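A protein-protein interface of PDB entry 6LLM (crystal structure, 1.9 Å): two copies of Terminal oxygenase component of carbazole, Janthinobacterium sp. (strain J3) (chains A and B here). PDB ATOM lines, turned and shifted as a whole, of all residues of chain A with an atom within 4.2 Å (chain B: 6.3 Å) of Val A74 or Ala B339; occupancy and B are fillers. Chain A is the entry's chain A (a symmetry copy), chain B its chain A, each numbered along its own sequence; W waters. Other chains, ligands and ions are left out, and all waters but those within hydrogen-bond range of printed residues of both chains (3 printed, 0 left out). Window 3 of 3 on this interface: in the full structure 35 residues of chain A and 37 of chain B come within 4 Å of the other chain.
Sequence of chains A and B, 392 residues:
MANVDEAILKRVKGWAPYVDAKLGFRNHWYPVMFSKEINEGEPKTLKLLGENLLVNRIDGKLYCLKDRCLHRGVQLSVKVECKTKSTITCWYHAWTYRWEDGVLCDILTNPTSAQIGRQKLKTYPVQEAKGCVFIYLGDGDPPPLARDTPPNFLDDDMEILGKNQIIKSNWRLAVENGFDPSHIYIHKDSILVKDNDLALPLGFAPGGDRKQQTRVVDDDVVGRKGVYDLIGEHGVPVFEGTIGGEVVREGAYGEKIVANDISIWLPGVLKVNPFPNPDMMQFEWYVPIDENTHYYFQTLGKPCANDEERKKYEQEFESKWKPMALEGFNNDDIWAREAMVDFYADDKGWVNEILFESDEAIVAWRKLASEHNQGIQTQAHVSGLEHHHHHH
Of chain B, only Ala B339 and Met B340 come within 4 Å of Val A74.
Ala B339 touches two residues of chain A.
Of the printed residues of chain A, Met B340 touches Arg A72 (3.9 Å), Val A74 (3.7 Å) and Tyr A92 (3.3 Å).
Of the printed residues of chain B, Trp A91 touches Trp B335 (3.4 Å), Ala B336 (3.8 Å) and Ala B339 (3.6 Å).
Ile B334 touches none of the printed residues of chain A.
The nearest printed residue of chain A that does not touch Ala B339 is Gly A73 (4.6 Å).
The nearest printed residue of chain B that does not touch Tyr A92 is Ala B336 (4.1 Å).
Among the printed residues, merely in contact across the chains: Arg A72 with Met B340 (3.9 Å), Arg A72 with Phe B343 (3.2 Å), Gly A73 with Phe B343 (3.5 Å), Val A74 with Ala B339 (3.6 Å), Val A74 with Met B340 (3.7 Å), Trp A91 with Trp B335 (3.4 Å), Trp A91 with Ala B336 (3.8 Å), Trp A91 with Ala B339 (3.6 Å) and Tyr A92 with Met B340 (3.3 Å).
Water W2 lies within hydrogen-bond range of the side-chain carboxylate of Asp B342 (2.6 Å) and the side-chain amide oxygen of Gln A75 (2.7 Å).
Water W3 bridges the backbone carbonyl oxygen (O) of Ala B339 and the backbone NH (N) of Gln A75.
Water W1 lies within hydrogen-bond range of the backbone carbonyl oxygen of Ala B339 (2.7 Å), the backbone NH of Phe B343 (2.9 Å), the backbone carbonyl oxygen of Gly A73 (3.0 Å) and the backbone NH of Asp B342 (3.4 Å).
Printed residues of chain B that touch a printed residue of chain A: Trp B335, Ala B336, Ala B339, Met B340 and Phe B343.
Of the 10 printed residues of chain A, 5 touch a printed residue of chain B.
Hydrophobic or aromatic side chains of chain A that line the printed part of chain B: Val A74, Trp A91 and Tyr A92.
Among the printed residues, 9 pairs touch across the chains.
Among the printed residues, no Asp or Glu carboxylate lies within 4 Å of a Lys or Arg side-chain nitrogen of the other chain.
No position is printed for both chains.
Of the 9 pairs that touch across the chains among the printed residues, none has its exchanged pair printed and touching as well.
SG of Cys A90 sits close to N of Tyr A92 (3.5 Å).
N of Cys A69 sits at hydrogen-bond distance from O of Val A74.
The indole nitrogen (NE1) of Trp A91 sits at hydrogen-bond distance from the backbone carbonyl oxygen (O) of Gln A75.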
ATOM      1  N   ARG A  68     -20.053  13.225  -7.249  1.00  0.00           N
ATOM      2  CA  ARG A  68     -19.687  14.497  -6.671  1.00  0.00           C
ATOM      3  C   ARG A  68     -18.171  14.662  -6.782  1.00  0.00           C
ATOM      4  O   ARG A  68     -17.422  13.991  -6.080  1.00  0.00           O
ATOM      5  CB  ARG A  68     -20.112  14.594  -5.212  1.00  0.00           C
ATOM      6  CG  ARG A  68     -20.008  16.004  -4.682  1.00  0.00           C
ATOM      7  CD  ARG A  68     -20.524  16.210  -3.269  1.00  0.00           C
ATOM      8  NE  ARG A  68     -19.773  15.333  -2.403  1.00  0.00           N
ATOM      9  CZ  ARG A  68     -20.233  14.763  -1.298  1.00  0.00           C
ATOM     10  NH1 ARG A  68     -21.414  15.093  -0.817  1.00  0.00           N
ATOM     11  NH2 ARG A  68     -19.526  13.807  -0.731  1.00  0.00           N
ATOM     12  N   CYS A  69     -17.748  15.582  -7.625  1.00  0.00           N
ATOM     13  CA  CYS A  69     -16.338  15.880  -7.809  1.00  0.00           C
ATOM     14  C   CYS A  69     -15.714  16.355  -6.504  1.00  0.00           C
ATOM     15  O   CYS A  69     -16.355  17.133  -5.733  1.00  0.00           O
ATOM     16  CB  CYS A  69     -16.177  16.936  -8.869  1.00  0.00           C
ATOM     17  SG  CYS A  69     -14.456  17.138  -9.384  1.00  0.00           S
ATOM     18  N   ARG A  72     -14.822  21.061  -6.561  1.00  0.00           N
ATOM     19  CA  ARG A  72     -15.814  22.060  -6.207  1.00  0.00           C
ATOM     20  C   ARG A  72     -17.173  21.436  -5.958  1.00  0.00           C
ATOM     21  O   ARG A  72     -18.154  22.161  -5.840  1.00  0.00           O
ATOM     22  CB  ARG A  72     -15.927  23.162  -7.264  1.00  0.00           C
ATOM     23  CG  ARG A  72     -14.622  23.894  -7.543  1.00  0.00           C
ATOM     24  CD  ARG A  72     -13.981  24.532  -6.350  1.00  0.00           C
ATOM     25  NE  ARG A  72     -14.751  25.589  -5.731  1.00  0.00           N
ATOM     26  CZ  ARG A  72     -14.855  26.866  -6.136  1.00  0.00           C
ATOM     27  NH1 ARG A  72     -14.120  27.357  -7.122  1.00  0.00           N
ATOM     28  NH2 ARG A  72     -15.677  27.662  -5.487  1.00  0.00           N
ATOM     29  N   GLY A  73     -17.249  20.114  -5.845  1.00  0.00           N
ATOM     30  CA  GLY A  73     -18.499  19.477  -5.348  1.00  0.00           C
ATOM     31  C   GLY A  73     -19.669  19.467  -6.330  1.00  0.00           C
ATOM     32  O   GLY A  73     -20.783  19.214  -5.951  1.00  0.00           O
ATOM     33  N   VAL A  74     -19.415  19.629  -7.624  1.00  0.00           N
ATOM     34  CA  VAL A  74     -20.462  19.509  -8.668  1.00  0.00           C
ATOM     35  C   VAL A  74     -20.726  18.041  -8.980  1.00  0.00           C
ATOM     36  O   VAL A  74     -19.883  17.132  -8.719  1.00  0.00           O
ATOM     37  CB  VAL A  74     -20.070  20.200  -9.973  1.00  0.00           C
ATOM     38  CG1 VAL A  74     -19.724  21.658  -9.767  1.00  0.00           C
ATOM     39  CG2 VAL A  74     -18.949  19.434 -10.664  1.00  0.00           C
ATOM     40  N   GLN A  75     -21.928  17.771  -9.465  1.00  0.00           N
ATOM     41  CA  GLN A  75     -22.221  16.453 -10.006  1.00  0.00           C
ATOM     42  C   GLN A  75     -21.495  16.299 -11.339  1.00  0.00           C
ATOM     43  O   GLN A  75     -21.681  17.088 -12.249  1.00  0.00           O
ATOM     44  CB  GLN A  75     -23.721  16.213 -10.146  1.00  0.00           C
ATOM     45  CG  GLN A  75     -24.359  15.844  -8.819  1.00  0.00           C
ATOM     46  CD  GLN A  75     -25.857  15.722  -8.909  1.00  0.00           C
ATOM     47  OE1 GLN A  75     -26.579  16.645  -8.527  1.00  0.00           O
ATOM     48  NE2 GLN A  75     -26.334  14.619  -9.461  1.00  0.00           N
ATOM     49  N   LEU A  76     -20.711  15.235 -11.471  1.00  0.00           N
ATOM     50  CA  LEU A  76     -20.089  14.892 -12.778  1.00  0.00           C
ATOM     51  C   LEU A  76     -21.183  14.688 -13.839  1.00  0.00           C
ATOM     52  O   LEU A  76     -21.003  15.008 -15.022  1.00  0.00           O
ATOM     53  CB  LEU A  76     -19.260  13.622 -12.611  1.00  0.00           C
ATOM     54  CG  LEU A  76     -18.242  13.614 -11.465  1.00  0.00           C
ATOM     55  CD1 LEU A  76     -17.683  12.216 -11.269  1.00  0.00           C
ATOM     56  CD2 LEU A  76     -17.078  14.582 -11.722  1.00  0.00           C
ATOM     57  N   CYS A  90     -14.410  15.026 -14.970  1.00  0.00           N
ATOM     58  CA  CYS A  90     -15.318  16.092 -14.602  1.00  0.00           C
ATOM     59  C   CYS A  90     -15.330  17.157 -15.702  1.00  0.00           C
ATOM     60  O   CYS A  90     -14.282  17.572 -16.197  1.00  0.00           O
ATOM     61  CB  CYS A  90     -14.886  16.740 -13.294  1.00  0.00           C
ATOM     62  SG  CYS A  90     -16.016  18.028 -12.688  1.00  0.00           S
ATOM     63  N   TRP A  91     -16.544  17.612 -16.051  1.00  0.00           N
ATOM     64  CA  TRP A  91     -16.790  18.616 -17.072  1.00  0.00           C
ATOM     65  C   TRP A  91     -16.251  19.994 -16.675  1.00  0.00           C
ATOM     66  O   TRP A  91     -16.122  20.865 -17.532  1.00  0.00           O
ATOM     67  CB  TRP A  91     -18.287  18.685 -17.373  1.00  0.00           C
ATOM     68  CG  TRP A  91     -19.095  19.000 -16.134  1.00  0.00           C
ATOM     69  CD1 TRP A  91     -19.725  18.091 -15.340  1.00  0.00           C
ATOM     70  CD2 TRP A  91     -19.327  20.282 -15.528  1.00  0.00           C
ATOM     71  NE1 TRP A  91     -20.260  18.709 -14.243  1.00  0.00           N
ATOM     72  CE2 TRP A  91     -20.039  20.055 -14.327  1.00  0.00           C
ATOM     73  CE3 TRP A  91     -18.917  21.597 -15.797  1.00  0.00           C
ATOM     74  CZ2 TRP A  91     -20.445  21.101 -13.484  1.00  0.00           C
ATOM     75  CZ3 TRP A  91     -19.308  22.631 -14.982  1.00  0.00           C
ATOM     76  CH2 TRP A  91     -20.019  22.369 -13.789  1.00  0.00           C
ATOM     77  N   TYR A  92     -15.932  20.232 -15.409  1.00  0.00           N
ATOM     78  CA  TYR A  92     -15.640  21.585 -14.996  1.00  0.00           C
ATOM     79  C   TYR A  92     -14.150  21.958 -15.140  1.00  0.00           C
ATOM     80  O   TYR A  92     -13.797  22.894 -15.850  1.00  0.00           O
ATOM     81  CB  TYR A  92     -16.185  21.766 -13.589  1.00  0.00           C
ATOM     82  CG  TYR A  92     -16.442  23.189 -13.175  1.00  0.00           C
ATOM     83  CD1 TYR A  92     -16.138  24.270 -13.972  1.00  0.00           C
ATOM     84  CD2 TYR A  92     -16.966  23.460 -11.894  1.00  0.00           C
ATOM     85  CE1 TYR A  92     -16.372  25.575 -13.530  1.00  0.00           C
ATOM     86  CE2 TYR A  92     -17.215  24.753 -11.461  1.00  0.00           C
ATOM     87  CZ  TYR A  92     -16.901  25.825 -12.266  1.00  0.00           C
ATOM     88  OH  TYR A  92     -17.108  27.123 -11.792  1.00  0.00           O
ATOM     89  N   ILE B 334     -23.115  30.026 -16.906  1.00  0.00           N
ATOM     90  CA  ILE B 334     -24.329  30.105 -16.121  1.00  0.00           C
ATOM     91  C   ILE B 334     -24.592  28.747 -15.498  1.00  0.00           C
ATOM     92  O   ILE B 334     -24.841  28.658 -14.295  1.00  0.00           O
ATOM     93  CB  ILE B 334     -25.506  30.622 -16.974  1.00  0.00           C
ATOM     94  CG1 ILE B 334     -25.265  32.081 -17.352  1.00  0.00           C
ATOM     95  CG2 ILE B 334     -26.827  30.408 -16.235  1.00  0.00           C
ATOM     96  CD1 ILE B 334     -26.272  32.669 -18.355  1.00  0.00           C
ATOM     97  N   TRP B 335     -24.610  27.691 -16.313  1.00  0.00           N
ATOM     98  CA  TRP B 335     -24.963  26.411 -15.760  1.00  0.00           C
ATOM     99  C   TRP B 335     -23.815  25.856 -14.879  1.00  0.00           C
ATOM    100  O   TRP B 335     -24.098  25.101 -13.959  1.00  0.00           O
ATOM    101  CB  TRP B 335     -25.492  25.400 -16.784  1.00  0.00           C
ATOM    102  CG  TRP B 335     -24.539  24.983 -17.847  1.00  0.00           C
ATOM    103  CD1 TRP B 335     -24.465  25.481 -19.119  1.00  0.00           C
ATOM    104  CD2 TRP B 335     -23.518  23.961 -17.759  1.00  0.00           C
ATOM    105  NE1 TRP B 335     -23.456  24.853 -19.810  1.00  0.00           N
ATOM    106  CE2 TRP B 335     -22.859  23.916 -19.014  1.00  0.00           C
ATOM    107  CE3 TRP B 335     -23.066  23.103 -16.748  1.00  0.00           C
ATOM    108  CZ2 TRP B 335     -21.769  23.078 -19.276  1.00  0.00           C
ATOM    109  CZ3 TRP B 335     -22.024  22.228 -17.026  1.00  0.00           C
ATOM    110  CH2 TRP B 335     -21.388  22.219 -18.276  1.00  0.00           C
ATOM    111  N   ALA B 336     -22.577  26.254 -15.124  1.00  0.00           N
ATOM    112  CA  ALA B 336     -21.433  25.891 -14.202  1.00  0.00           C
ATOM    113  C   ALA B 336     -21.688  26.487 -12.816  1.00  0.00           C
ATOM    114  O   ALA B 336     -21.560  25.799 -11.787  1.00  0.00           O
ATOM    115  CB  ALA B 336     -20.136  26.354 -14.809  1.00  0.00           C
ATOM    116  N   ARG B 337     -22.094  27.767 -12.767  1.00  0.00           N
ATOM    117  CA  ARG B 337     -22.383  28.388 -11.467  1.00  0.00           C
ATOM    118  C   ARG B 337     -23.472  27.587 -10.763  1.00  0.00           C
ATOM    119  O   ARG B 337     -23.385  27.308  -9.578  1.00  0.00           O
ATOM    120  CB  ARG B 337     -22.936  29.808 -11.644  1.00  0.00           C
ATOM    121  CG  ARG B 337     -21.920  30.775 -12.177  1.00  0.00           C
ATOM    122  CD  ARG B 337     -22.685  32.028 -12.664  1.00  0.00           C
ATOM    123  NE  ARG B 337     -21.781  32.810 -13.438  1.00  0.00           N
ATOM    124  CZ  ARG B 337     -22.184  33.790 -14.234  1.00  0.00           C
ATOM    125  NH1 ARG B 337     -23.347  34.368 -13.985  1.00  0.00           N
ATOM    126  NH2 ARG B 337     -21.385  34.192 -15.189  1.00  0.00           N
ATOM    127  N   GLU B 338     -24.534  27.272 -11.508  1.00  0.00           N
ATOM    128  CA  GLU B 338     -25.681  26.611 -10.998  1.00  0.00           C
ATOM    129  C   GLU B 338     -25.323  25.250 -10.375  1.00  0.00           C
ATOM    130  O   GLU B 338     -25.924  24.814  -9.371  1.00  0.00           O
ATOM    131  CB  GLU B 338     -26.745  26.527 -12.074  1.00  0.00           C
ATOM    132  CG  GLU B 338     -27.421  27.878 -12.345  1.00  0.00           C
ATOM    133  CD  GLU B 338     -28.400  27.809 -13.504  1.00  0.00           C
ATOM    134  OE1 GLU B 338     -28.165  27.024 -14.467  1.00  0.00           O
ATOM    135  OE2 GLU B 338     -29.386  28.502 -13.442  1.00  0.00           O
ATOM    136  N   ALA B 339     -24.358  24.578 -10.985  1.00  0.00           N
ATOM    137  CA  ALA B 339     -23.939  23.229 -10.562  1.00  0.00           C
ATOM    138  C   ALA B 339     -23.169  23.254  -9.244  1.00  0.00           C
ATOM    139  O   ALA B 339     -23.074  22.197  -8.571  1.00  0.00           O
ATOM    140  CB  ALA B 339     -23.144  22.605 -11.657  1.00  0.00           C
ATOM    141  N   MET B 340     -22.697  24.421  -8.809  1.00  0.00           N
ATOM    142  CA  MET B 340     -21.987  24.483  -7.525  1.00  0.00           C
ATOM    143  C   MET B 340     -22.943  24.815  -6.371  1.00  0.00           C
ATOM    144  O   MET B 340     -22.547  24.726  -5.223  1.00  0.00           O
ATOM    145  CB  MET B 340     -20.857  25.518  -7.528  1.00  0.00           C
ATOM    146  CG  MET B 340     -19.588  25.051  -8.213  1.00  0.00           C
ATOM    147  SD  MET B 340     -18.239  26.248  -8.022  1.00  0.00           S
ATOM    148  CE  MET B 340     -18.876  27.606  -9.007  1.00  0.00           C
ATOM    149  N   VAL B 341     -24.211  25.131  -6.688  1.00  0.00           N
ATOM    150  CA  VAL B 341     -25.143  25.597  -5.670  1.00  0.00           C
ATOM    151  C   VAL B 341     -25.270  24.593  -4.535  1.00  0.00           C
ATOM    152  O   VAL B 341     -25.101  24.971  -3.385  1.00  0.00           O
ATOM    153  CB  VAL B 341     -26.510  25.971  -6.275  1.00  0.00           C
ATOM    154  CG1 VAL B 341     -27.570  26.145  -5.196  1.00  0.00           C
ATOM    155  CG2 VAL B 341     -26.358  27.228  -7.105  1.00  0.00           C
ATOM    156  N   ASP B 342     -25.472  23.321  -4.869  1.00  0.00           N
ATOM    157  CA  ASP B 342     -25.799  22.345  -3.817  1.00  0.00           C
ATOM    158  C   ASP B 342     -24.657  22.180  -2.812  1.00  0.00           C
ATOM    159  O   ASP B 342     -24.878  22.090  -1.625  1.00  0.00           O
ATOM    160  CB  ASP B 342     -26.136  20.975  -4.398  1.00  0.00           C
ATOM    161  CG  ASP B 342     -27.418  20.924  -5.226  1.00  0.00           C
ATOM    162  OD1 ASP B 342     -28.320  21.839  -5.048  1.00  0.00           O
ATOM    163  OD2 ASP B 342     -27.455  20.077  -6.144  1.00  0.00           O
ATOM    164  N   PHE B 343     -23.419  22.095  -3.292  1.00  0.00           N
ATOM    165  CA  PHE B 343     -22.283  21.911  -2.425  1.00  0.00           C
ATOM    166  C   PHE B 343     -22.056  23.087  -1.475  1.00  0.00           C
ATOM    167  O   PHE B 343     -21.549  22.879  -0.362  1.00  0.00           O
ATOM    168  CB  PHE B 343     -21.060  21.655  -3.312  1.00  0.00           C
ATOM    169  CG  PHE B 343     -19.873  21.132  -2.573  1.00  0.00           C
ATOM    170  CD1 PHE B 343     -19.953  19.934  -1.871  1.00  0.00           C
ATOM    171  CD2 PHE B 343     -18.666  21.805  -2.651  1.00  0.00           C
ATOM    172  CE1 PHE B 343     -18.830  19.428  -1.231  1.00  0.00           C
ATOM    173  CE2 PHE B 343     -17.541  21.276  -2.028  1.00  0.00           C
ATOM    174  CZ  PHE B 343     -17.647  20.122  -1.287  1.00  0.00           C
HETATM  175  O   HOH W   1     -23.010  21.245  -6.022  1.00  0.00           O
HETATM  176  O   HOH W   2     -25.460  18.599  -7.031  1.00  0.00           O
HETATM  177  O   HOH W   3     -24.035  19.760  -9.296  1.00  0.00           O
